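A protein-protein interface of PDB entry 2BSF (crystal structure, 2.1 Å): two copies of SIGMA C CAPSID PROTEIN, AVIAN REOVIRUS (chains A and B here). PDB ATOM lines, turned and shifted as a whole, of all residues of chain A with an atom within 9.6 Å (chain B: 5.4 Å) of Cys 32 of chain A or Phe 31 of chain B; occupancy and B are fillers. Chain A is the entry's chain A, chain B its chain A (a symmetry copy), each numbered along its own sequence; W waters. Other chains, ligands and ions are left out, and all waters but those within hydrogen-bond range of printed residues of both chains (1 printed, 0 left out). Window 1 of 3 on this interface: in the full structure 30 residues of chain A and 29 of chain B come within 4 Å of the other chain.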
ATOM      1  N   PRO A  15      13.648  12.487   0.519  1.00  0.00           N
ATOM      2  CA  PRO A  15      13.346  11.081   0.824  1.00  0.00           C
ATOM      3  C   PRO A  15      12.894  10.226  -0.369  1.00  0.00           C
ATOM      4  O   PRO A  15      12.433   9.102  -0.159  1.00  0.00           O
ATOM      5  CB  PRO A  15      12.196  11.200   1.827  1.00  0.00           C
ATOM      6  CG  PRO A  15      11.474  12.419   1.353  1.00  0.00           C
ATOM      7  CD  PRO A  15      12.495  13.359   0.809  1.00  0.00           C
ATOM      8  N   LEU A  25       9.362   6.344  -2.102  1.00  0.00           N
ATOM      9  CA  LEU A  25       9.473   7.306  -0.991  1.00  0.00           C
ATOM     10  C   LEU A  25       9.919   6.533   0.254  1.00  0.00           C
ATOM     11  O   LEU A  25       9.237   5.634   0.710  1.00  0.00           O
ATOM     12  CB  LEU A  25       8.135   8.021  -0.729  1.00  0.00           C
ATOM     13  CG  LEU A  25       8.045   8.956   0.488  1.00  0.00           C
ATOM     14  CD1 LEU A  25       8.799  10.247   0.199  1.00  0.00           C
ATOM     15  CD2 LEU A  25       6.585   9.232   0.892  1.00  0.00           C
ATOM     16  N   ASP A  26      11.091   6.872   0.774  1.00  0.00           N
ATOM     17  CA  ASP A  26      11.545   6.366   2.057  1.00  0.00           C
ATOM     18  C   ASP A  26      10.771   7.015   3.233  1.00  0.00           C
ATOM     19  O   ASP A  26      10.758   8.222   3.361  1.00  0.00           O
ATOM     20  CB  ASP A  26      13.046   6.638   2.169  1.00  0.00           C
ATOM     21  CG  ASP A  26      13.835   5.899   1.088  1.00  0.00           C
ATOM     22  OD1 ASP A  26      13.514   4.714   0.847  1.00  0.00           O
ATOM     23  OD2 ASP A  26      14.761   6.494   0.500  1.00  0.00           O
ATOM     24  N   MET A  27      10.157   6.201   4.083  1.00  0.00           N
ATOM     25  CA  MET A  27       9.261   6.691   5.125  1.00  0.00           C
ATOM     26  C   MET A  27       9.778   6.285   6.498  1.00  0.00           C
ATOM     27  O   MET A  27      10.079   5.120   6.726  1.00  0.00           O
ATOM     28  CB  MET A  27       7.890   6.116   4.882  1.00  0.00           C
ATOM     29  CG  MET A  27       7.212   6.682   3.630  1.00  0.00           C
ATOM     30  SD  MET A  27       5.790   5.681   3.178  1.00  0.00           S
ATOM     31  CE  MET A  27       6.510   4.096   2.703  1.00  0.00           C
ATOM     32  N   ASP A  28       9.924   7.255   7.404  1.00  0.00           N
ATOM     33  CA  ASP A  28      10.248   6.952   8.796  1.00  0.00           C
ATOM     34  C   ASP A  28       8.971   6.322   9.406  1.00  0.00           C
ATOM     35  O   ASP A  28       7.959   6.981   9.482  1.00  0.00           O
ATOM     36  CB  ASP A  28      10.653   8.262   9.483  1.00  0.00           C
ATOM     37  CG  ASP A  28      10.520   8.222  11.026  1.00  0.00           C
ATOM     38  OD1 ASP A  28      10.556   7.130  11.625  1.00  0.00           O
ATOM     39  OD2 ASP A  28      10.445   9.323  11.636  1.00  0.00           O
ATOM     40  N   PRO A  29       9.016   5.046   9.832  1.00  0.00           N
ATOM     41  CA  PRO A  29       7.745   4.460  10.207  1.00  0.00           C
ATOM     42  C   PRO A  29       7.114   5.070  11.504  1.00  0.00           C
ATOM     43  O   PRO A  29       5.922   4.847  11.741  1.00  0.00           O
ATOM     44  CB  PRO A  29       8.084   2.982  10.392  1.00  0.00           C
ATOM     45  CG  PRO A  29       9.538   2.978  10.806  1.00  0.00           C
ATOM     46  CD  PRO A  29      10.147   4.112  10.028  1.00  0.00           C
ATOM     47  N   TYR A  30       7.903   5.819  12.296  1.00  0.00           N
ATOM     48  CA  TYR A  30       7.375   6.584  13.469  1.00  0.00           C
ATOM     49  C   TYR A  30       6.545   7.831  13.068  1.00  0.00           C
ATOM     50  O   TYR A  30       5.838   8.429  13.895  1.00  0.00           O
ATOM     51  CB  TYR A  30       8.520   6.952  14.451  1.00  0.00           C
ATOM     52  CG  TYR A  30       9.087   5.742  15.140  1.00  0.00           C
ATOM     53  CD1 TYR A  30       8.480   5.224  16.290  1.00  0.00           C
ATOM     54  CD2 TYR A  30      10.221   5.074  14.628  1.00  0.00           C
ATOM     55  CE1 TYR A  30       8.954   4.083  16.886  1.00  0.00           C
ATOM     56  CE2 TYR A  30      10.712   3.921  15.241  1.00  0.00           C
ATOM     57  CZ  TYR A  30      10.079   3.440  16.372  1.00  0.00           C
ATOM     58  OH  TYR A  30      10.550   2.324  17.029  1.00  0.00           O
ATOM     59  N   PHE A  31       6.612   8.215  11.797  1.00  0.00           N
ATOM     60  CA  PHE A  31       5.927   9.380  11.313  1.00  0.00           C
ATOM     61  C   PHE A  31       4.885   9.067  10.251  1.00  0.00           C
ATOM     62  O   PHE A  31       3.797   9.621  10.290  1.00  0.00           O
ATOM     63  CB  PHE A  31       6.934  10.427  10.781  1.00  0.00           C
ATOM     64  CG  PHE A  31       6.271  11.631  10.171  1.00  0.00           C
ATOM     65  CD1 PHE A  31       5.546  12.522  10.971  1.00  0.00           C
ATOM     66  CD2 PHE A  31       6.328  11.856   8.805  1.00  0.00           C
ATOM     67  CE1 PHE A  31       4.918  13.645  10.420  1.00  0.00           C
ATOM     68  CE2 PHE A  31       5.694  12.988   8.229  1.00  0.00           C
ATOM     69  CZ  PHE A  31       4.995  13.874   9.024  1.00  0.00           C
ATOM     70  N   CYS A  32       5.199   8.178   9.303  1.00  0.00           N
ATOM     71  CA  CYS A  32       4.300   7.963   8.168  1.00  0.00           C
ATOM     72  C   CYS A  32       4.477   6.569   7.613  1.00  0.00           C
ATOM     73  O   CYS A  32       5.378   5.856   8.012  1.00  0.00           O
ATOM     74  CB  CYS A  32       4.508   8.998   7.051  1.00  0.00           C
ATOM     75  SG  CYS A  32       6.176   9.015   6.290  1.00  0.00           S
ATOM     76  N   SER A  33       3.575   6.188   6.721  1.00  0.00           N
ATOM     77  CA  SER A  33       3.563   4.858   6.122  1.00  0.00           C
ATOM     78  C   SER A  33       2.684   4.958   4.889  1.00  0.00           C
ATOM     79  O   SER A  33       2.142   6.031   4.589  1.00  0.00           O
ATOM     80  CB  SER A  33       2.981   3.831   7.104  1.00  0.00           C
ATOM     81  OG  SER A  33       1.615   4.116   7.336  1.00  0.00           O
ATOM     82  N   GLN A  34       2.532   3.857   4.164  1.00  0.00           N
ATOM     83  CA  GLN A  34       1.654   3.879   3.008  1.00  0.00           C
ATOM     84  C   GLN A  34       0.600   2.812   3.177  1.00  0.00           C
ATOM     85  O   GLN A  34       0.893   1.706   3.609  1.00  0.00           O
ATOM     86  CB  GLN A  34       2.400   3.758   1.664  1.00  0.00           C
ATOM     87  CG  GLN A  34       3.133   2.419   1.349  1.00  0.00           C
ATOM     88  CD  GLN A  34       2.210   1.274   0.913  1.00  0.00           C
ATOM     89  OE1 GLN A  34       1.086   1.487   0.436  1.00  0.00           O
ATOM     90  NE2 GLN A  34       2.684   0.045   1.100  1.00  0.00           N
ATOM     91  N   ARG A  35      -0.640   3.180   2.887  1.00  0.00           N
ATOM     92  CA  ARG A  35      -1.705   2.205   2.703  1.00  0.00           C
ATOM     93  C   ARG A  35      -2.341   2.658   1.416  1.00  0.00           C
ATOM     94  O   ARG A  35      -3.411   3.252   1.427  1.00  0.00           O
ATOM     95  CB  ARG A  35      -2.706   2.197   3.868  1.00  0.00           C
ATOM     96  CG  ARG A  35      -2.035   2.063   5.243  1.00  0.00           C
ATOM     97  CD  ARG A  35      -2.832   1.265   6.268  1.00  0.00           C
ATOM     98  NE  ARG A  35      -2.055   1.160   7.509  1.00  0.00           N
ATOM     99  CZ  ARG A  35      -2.021   0.095   8.316  1.00  0.00           C
ATOM    100  NH1 ARG A  35      -2.727  -0.997   8.023  1.00  0.00           N
ATOM    101  NH2 ARG A  35      -1.274   0.120   9.426  1.00  0.00           N
ATOM    102  N   SER A  37      -2.108   5.257  -0.135  1.00  0.00           N
ATOM    103  CA  SER A  37      -1.759   6.655   0.029  1.00  0.00           C
ATOM    104  C   SER A  37      -0.818   6.867   1.217  1.00  0.00           C
ATOM    105  O   SER A  37      -0.695   5.996   2.087  1.00  0.00           O
ATOM    106  CB  SER A  37      -3.034   7.489   0.196  1.00  0.00           C
ATOM    107  OG  SER A  37      -3.765   7.027   1.317  1.00  0.00           O
ATOM    108  N   LEU A  38      -0.150   8.018   1.243  1.00  0.00           N
ATOM    109  CA  LEU A  38       0.748   8.363   2.319  1.00  0.00           C
ATOM    110  C   LEU A  38      -0.111   8.732   3.543  1.00  0.00           C
ATOM    111  O   LEU A  38      -0.906   9.646   3.483  1.00  0.00           O
ATOM    112  CB  LEU A  38       1.654   9.559   1.950  1.00  0.00           C
ATOM    113  CG  LEU A  38       2.675  10.012   3.027  1.00  0.00           C
ATOM    114  CD1 LEU A  38       3.759   8.947   3.308  1.00  0.00           C
ATOM    115  CD2 LEU A  38       3.325  11.319   2.639  1.00  0.00           C
ATOM    116  N   THR A  39       0.088   8.020   4.638  1.00  0.00           N
ATOM    117  CA  THR A  39      -0.679   8.215   5.875  1.00  0.00           C
ATOM    118  C   THR A  39       0.262   8.216   7.111  1.00  0.00           C
ATOM    119  O   THR A  39       1.497   8.255   6.982  1.00  0.00           O
ATOM    120  CB  THR A  39      -1.811   7.147   5.978  1.00  0.00           C
ATOM    121  OG1 THR A  39      -2.684   7.440   7.082  1.00  0.00           O
ATOM    122  CG2 THR A  39      -1.222   5.733   6.086  1.00  0.00           C
ATOM    123  N   SER A  40      -0.329   8.162   8.299  1.00  0.00           N
ATOM    124  CA  SER A  40       0.403   8.360   9.550  1.00  0.00           C
ATOM    125  C   SER A  40       1.176   7.127   9.960  1.00  0.00           C
ATOM    126  O   SER A  40       1.223   6.140   9.222  1.00  0.00           O
ATOM    127  CB  SER A  40      -0.542   8.836  10.664  1.00  0.00           C
ATOM    128  OG  SER A  40      -1.590   7.915  10.802  1.00  0.00           O
ATOM    129  N   TYR A  41       1.788   7.184  11.142  1.00  0.00           N
ATOM    130  CA  TYR A  41       2.802   6.225  11.519  1.00  0.00           C
ATOM    131  C   TYR A  41       2.333   4.774  11.560  1.00  0.00           C
ATOM    132  O   TYR A  41       1.190   4.470  11.915  1.00  0.00           O
ATOM    133  CB  TYR A  41       3.422   6.611  12.859  1.00  0.00           C
ATOM    134  CG  TYR A  41       2.473   6.487  14.062  1.00  0.00           C
ATOM    135  CD1 TYR A  41       2.401   5.287  14.795  1.00  0.00           C
ATOM    136  CD2 TYR A  41       1.706   7.586  14.494  1.00  0.00           C
ATOM    137  CE1 TYR A  41       1.559   5.171  15.913  1.00  0.00           C
ATOM    138  CE2 TYR A  41       0.860   7.496  15.615  1.00  0.00           C
ATOM    139  CZ  TYR A  41       0.800   6.290  16.307  1.00  0.00           C
ATOM    140  OH  TYR A  41       0.002   6.169  17.387  1.00  0.00           O
ATOM    141  N   SER A  42       3.265   3.866  11.277  1.00  0.00           N
ATOM    142  CA  SER A  42       2.974   2.445  11.394  1.00  0.00           C
ATOM    143  C   SER A  42       3.714   1.801  12.579  1.00  0.00           C
ATOM    144  O   SER A  42       3.374   0.697  13.001  1.00  0.00           O
ATOM    145  CB  SER A  42       3.376   1.715  10.087  1.00  0.00           C
ATOM    146  OG  SER A  42       4.761   1.912   9.845  1.00  0.00           O
ATOM    147  N   ALA A  43       4.746   2.458  13.098  1.00  0.00           N
ATOM    148  CA  ALA A  43       5.490   1.888  14.219  1.00  0.00           C
ATOM    149  C   ALA A  43       4.583   1.684  15.427  1.00  0.00           C
ATOM    150  O   ALA A  43       3.678   2.482  15.689  1.00  0.00           O
ATOM    151  CB  ALA A  43       6.659   2.782  14.603  1.00  0.00           C
ATOM    152  N   GLY A  74       3.863   7.283  17.726  1.00  0.00           N
ATOM    153  CA  GLY A  74       4.431   8.054  16.631  1.00  0.00           C
ATOM    154  C   GLY A  74       5.663   8.778  17.167  1.00  0.00           C
ATOM    155  O   GLY A  74       6.396   8.269  18.042  1.00  0.00           O
ATOM    156  N   ARG A  75       5.854  10.000  16.716  1.00  0.00           N
ATOM    157  CA  ARG A  75       6.963  10.784  17.241  1.00  0.00           C
ATOM    158  C   ARG A  75       6.525  11.692  18.398  1.00  0.00           C
ATOM    159  O   ARG A  75       7.182  12.670  18.715  1.00  0.00           O
ATOM    160  CB  ARG A  75       7.638  11.545  16.130  1.00  0.00           C
ATOM    161  CG  ARG A  75       8.051  10.621  14.960  1.00  0.00           C
ATOM    162  CD  ARG A  75       9.156  11.265  14.128  1.00  0.00           C
ATOM    163  NE  ARG A  75      10.391  11.328  14.900  1.00  0.00           N
ATOM    164  CZ  ARG A  75      11.362  10.409  14.922  1.00  0.00           C
ATOM    165  NH1 ARG A  75      11.304   9.308  14.191  1.00  0.00           N
ATOM    166  NH2 ARG A  75      12.415  10.600  15.706  1.00  0.00           N
ATOM    167  N   ASP B  28      -3.243  10.565   1.919  1.00  0.00           N
ATOM    168  CA  ASP B  28      -4.433  10.348   2.738  1.00  0.00           C
ATOM    169  C   ASP B  28      -4.844  11.741   3.275  1.00  0.00           C
ATOM    170  O   ASP B  28      -4.094  12.341   4.010  1.00  0.00           O
ATOM    171  CB  ASP B  28      -4.067   9.362   3.855  1.00  0.00           C
ATOM    172  CG  ASP B  28      -5.017   9.427   5.077  1.00  0.00           C
ATOM    173  OD1 ASP B  28      -6.177   9.861   4.941  1.00  0.00           O
ATOM    174  OD2 ASP B  28      -4.594   8.967   6.172  1.00  0.00           O
ATOM    175  N   PRO B  29      -6.030  12.258   2.901  1.00  0.00           N
ATOM    176  CA  PRO B  29      -6.263  13.638   3.277  1.00  0.00           C
ATOM    177  C   PRO B  29      -6.437  13.864   4.817  1.00  0.00           C
ATOM    178  O   PRO B  29      -6.352  15.016   5.258  1.00  0.00           O
ATOM    179  CB  PRO B  29      -7.538  13.996   2.514  1.00  0.00           C
ATOM    180  CG  PRO B  29      -8.274  12.683   2.375  1.00  0.00           C
ATOM    181  CD  PRO B  29      -7.184  11.664   2.191  1.00  0.00           C
ATOM    182  N   TYR B  30      -6.659  12.785   5.591  1.00  0.00           N
ATOM    183  CA  TYR B  30      -6.678  12.854   7.085  1.00  0.00           C
ATOM    184  C   TYR B  30      -5.272  13.048   7.711  1.00  0.00           C
ATOM    185  O   TYR B  30      -5.134  13.370   8.902  1.00  0.00           O
ATOM    186  CB  TYR B  30      -7.404  11.623   7.689  1.00  0.00           C
ATOM    187  CG  TYR B  30      -8.878  11.632   7.391  1.00  0.00           C
ATOM    188  CD1 TYR B  30      -9.767  12.354   8.198  1.00  0.00           C
ATOM    189  CD2 TYR B  30      -9.403  10.948   6.272  1.00  0.00           C
ATOM    190  CE1 TYR B  30     -11.102  12.419   7.894  1.00  0.00           C
ATOM    191  CE2 TYR B  30     -10.763  11.004   5.970  1.00  0.00           C
ATOM    192  CZ  TYR B  30     -11.605  11.732   6.790  1.00  0.00           C
ATOM    193  OH  TYR B  30     -12.960  11.786   6.549  1.00  0.00           O
ATOM    194  N   PHE B  31      -4.226  12.876   6.908  1.00  0.00           N
ATOM    195  CA  PHE B  31      -2.875  12.981   7.378  1.00  0.00           C
ATOM    196  C   PHE B  31      -2.091  14.100   6.710  1.00  0.00           C
ATOM    197  O   PHE B  31      -1.367  14.818   7.385  1.00  0.00           O
ATOM    198  CB  PHE B  31      -2.129  11.636   7.213  1.00  0.00           C
ATOM    199  CG  PHE B  31      -0.678  11.711   7.599  1.00  0.00           C
ATOM    200  CD1 PHE B  31      -0.310  11.916   8.934  1.00  0.00           C
ATOM    201  CD2 PHE B  31       0.318  11.622   6.639  1.00  0.00           C
ATOM    202  CE1 PHE B  31       1.036  11.993   9.311  1.00  0.00           C
ATOM    203  CE2 PHE B  31       1.687  11.701   7.004  1.00  0.00           C
ATOM    204  CZ  PHE B  31       2.045  11.887   8.324  1.00  0.00           C
ATOM    205  N   CYS B  32      -2.232  14.267   5.392  1.00  0.00           N
ATOM    206  CA  CYS B  32      -1.380  15.218   4.674  1.00  0.00           C
ATOM    207  C   CYS B  32      -2.079  15.716   3.431  1.00  0.00           C
ATOM    208  O   CYS B  32      -3.129  15.218   3.071  1.00  0.00           O
ATOM    209  CB  CYS B  32      -0.016  14.617   4.299  1.00  0.00           C
ATOM    210  SG  CYS B  32      -0.074  13.159   3.189  1.00  0.00           S
ATOM    211  N   SER B  33      -1.496  16.734   2.814  1.00  0.00           N
ATOM    212  CA  SER B  33      -2.061  17.374   1.632  1.00  0.00           C
ATOM    213  C   SER B  33      -0.932  18.170   1.003  1.00  0.00           C
ATOM    214  O   SER B  33       0.193  18.181   1.522  1.00  0.00           O
ATOM    215  CB  SER B  33      -3.213  18.311   2.024  1.00  0.00           C
ATOM    216  OG  SER B  33      -2.708  19.388   2.791  1.00  0.00           O
ATOM    217  N   THR B  39       2.244  19.109   3.286  1.00  0.00           N
ATOM    218  CA  THR B  39       1.860  19.646   4.598  1.00  0.00           C
ATOM    219  C   THR B  39       0.780  18.750   5.263  1.00  0.00           C
ATOM    220  O   THR B  39       0.484  17.638   4.794  1.00  0.00           O
ATOM    221  CB  THR B  39       1.408  21.133   4.456  1.00  0.00           C
ATOM    222  OG1 THR B  39       1.211  21.726   5.751  1.00  0.00           O
ATOM    223  CG2 THR B  39       0.146  21.243   3.589  1.00  0.00           C
ATOM    224  N   SER B  40       0.191  19.246   6.347  1.00  0.00           N
ATOM    225  CA  SER B  40      -0.689  18.444   7.197  1.00  0.00           C
ATOM    226  C   SER B  40      -2.072  18.295   6.604  1.00  0.00           C
ATOM    227  O   SER B  40      -2.325  18.734   5.480  1.00  0.00           O
ATOM    228  CB  SER B  40      -0.740  19.019   8.621  1.00  0.00           C
ATOM    229  OG  SER B  40      -1.136  20.362   8.561  1.00  0.00           O
ATOM    230  N   TYR B  41      -2.971  17.668   7.363  1.00  0.00           N
ATOM    231  CA  TYR B  41      -4.218  17.182   6.816  1.00  0.00           C
ATOM    232  C   TYR B  41      -5.119  18.253   6.211  1.00  0.00           C
ATOM    233  O   TYR B  41      -5.182  19.393   6.684  1.00  0.00           O
ATOM    234  CB  TYR B  41      -4.984  16.392   7.874  1.00  0.00           C
ATOM    235  CG  TYR B  41      -5.515  17.237   9.043  1.00  0.00           C
ATOM    236  CD1 TYR B  41      -6.800  17.809   8.987  1.00  0.00           C
ATOM    237  CD2 TYR B  41      -4.755  17.403  10.218  1.00  0.00           C
ATOM    238  CE1 TYR B  41      -7.305  18.560  10.062  1.00  0.00           C
ATOM    239  CE2 TYR B  41      -5.243  18.144  11.309  1.00  0.00           C
ATOM    240  CZ  TYR B  41      -6.511  18.712  11.214  1.00  0.00           C
ATOM    241  OH  TYR B  41      -7.011  19.426  12.242  1.00  0.00           O
ATOM    242  N   GLY B  74      -7.696  15.468  11.890  1.00  0.00           N
ATOM    243  CA  GLY B  74      -6.650  14.664  11.275  1.00  0.00           C
ATOM    244  C   GLY B  74      -6.876  13.214  11.696  1.00  0.00           C
ATOM    245  O   GLY B  74      -8.022  12.751  11.871  1.00  0.00           O
ATOM    246  N   ARG B  75      -5.790  12.513  11.946  1.00  0.00           N
ATOM    247  CA  ARG B  75      -5.925  11.147  12.430  1.00  0.00           C
ATOM    248  C   ARG B  75      -5.861  11.072  13.961  1.00  0.00           C
ATOM    249  O   ARG B  75      -5.581  10.030  14.530  1.00  0.00           O
ATOM    250  CB  ARG B  75      -4.911  10.253  11.762  1.00  0.00           C
ATOM    251  CG  ARG B  75      -4.970  10.358  10.221  1.00  0.00           C
ATOM    252  CD  ARG B  75      -4.354   9.121   9.572  1.00  0.00           C
ATOM    253  NE  ARG B  75      -5.196   7.957   9.818  1.00  0.00           N
ATOM    254  CZ  ARG B  75      -6.179   7.506   9.030  1.00  0.00           C
ATOM    255  NH1 ARG B  75      -6.483   8.090   7.883  1.00  0.00           N
ATOM    256  NH2 ARG B  75      -6.878   6.445   9.412  1.00  0.00           N
HETATM  257  O   HOH W   1      -4.183   5.213   7.752  1.00  0.00           O
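O of Leu 38 of chain A is in hydrogen-bond range of SG of Cys 32 of chain B. The side-chain hydroxyl (OG1) of Thr 39 of chain A lies within hydrogen-bond range of the side-chain carboxylate (OD2) of Asp 28 of chain B, at 2.6 Å. O of Leu 38 of chain A sits at hydrogen-bond distance from N of Asp 28 of chain B (3.0 Å).
The backbone carbonyl oxygen of Phe 31 of chain B lies within hydrogen-bond range of the backbone NH of Tyr 41 of chain B. OD2 of Asp 28 of chain B lies within salt-bridge range of NH1 of Arg 75 of chain B, at 2.7 Å. N of Thr 39 of chain A lies within hydrogen-bond range of O of Ser 33 of chain A, 2.9 Å away. The backbone carbonyl oxygen (O) of Phe 31 of chain A sits at hydrogen-bond distance from the backbone NH (N) of Tyr 41 of chain A (3.3 Å). N of Arg 75 of chain B is in hydrogen-bond range of O of Tyr 30 of chain B (3.2 Å). OG of Ser 33 of chain A lies within hydrogen-bond range of O of Ser 40 of chain A, 2.8 Å away.
Water W1 lies within hydrogen-bond range of OG1 of Thr 39 of chain A (2.8 Å) and NH2 of Arg 75 of chain B (3.4 Å).
Of the 11 printed residues of chain B, 4 touch a printed residue of chain A. Hydrophobic or aromatic side chains of chain B within 4 Å of the printed part of chain A: Phe 31. Of the 21 printed residues of chain A, 6 touch a printed residue of chain B. Hydrophobic or aromatic side chains of chain A that line the printed part of chain B: Phe 31 and Leu 38. Among the printed residues, 11 pairs touch across the chains. Among the printed residues, no Asp or Glu carboxylate lies within 4 Å of a Lys or Arg side-chain nitrogen of the other chain.
Phe 31 of chain A touches its own counterpart, Phe 31 of chain B. Thr 39 of chain A touches Asp 28 of chain B, but with the chains exchanged Asp 28 of chain A does not touch Thr 39 of chain B (13.8 Å). Thr 39 of chain A touches Arg 75 of chain B, but with the chains exchanged Arg 75 of chain A does not touch Thr 39 of chain B (14.2 Å). Ser 40 of chain A touches Arg 75 of chain B, but with the chains exchanged Arg 75 of chain A does not touch Ser 40 of chain B (13.5 Å). Positions printed for both chains: 28, 29, 30, 31, 32, 33, 39, 40, 41, 74 and 75. Of the 11 pairs that touch across the chains among the printed residues, 1 has its exchanged pair printed and touching as well.
Phe 31 of chain B touches Phe 31 of chain A (CZ to O, 3.5 Å). Phe 31 of chain B touches Cys 32 of chain A (CE2 to CB, 3.9 Å). OG of Ser 37 of chain A touches CB of Asp 28 of chain B, 3.5 Å away. Phe 31 of chain B touches Leu 38 of chain A (CD2 to O, 3.9 Å). C of Thr 39 of chain A touches CD2 of Phe 31 of chain B, 3.4 Å away. Thr 39 of chain A touches Arg 75 of chain B (OG1 to CD, 3.4 Å). Ser 40 of chain A touches Phe 31 of chain B. OG of Ser 40 of chain A touches CD of Arg 75 of chain B, at 3.3 Å.
Printed residues of chain B within 4 Å of Phe 31 of chain A: Phe 31 (3.5 Å). Cys 32 of chain A touches one residue of chain B. Of the printed residues of chain B, Ser 37 of chain A touches Asp 28. Of the printed residues of chain B, Leu 38 of chain A touches Asp 28, Phe 31 and Cys 32. Ser 42 of chain A touches none of the printed residues of chain B. Of the printed residues of chain A, Phe 31 of chain B touches Phe 31 (3.5 Å), Cys 32 (3.9 Å), Leu 38 (3.9 Å), Thr 39 (3.4 Å) and Ser 40 (3.5 Å). Cys 32 of chain B touches just one residue of chain A: Leu 38. Printed residues of chain A within 4 Å of Arg 75 of chain B: Thr 39 and Ser 40. The nearest printed residue of chain B that does not touch Cys 32 of chain A is Cys 32 of chain B (7.3 Å). The nearest residue of chain A that does not touch Phe 31 of chain B is Tyr 41 of chain A (5.2 Å).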
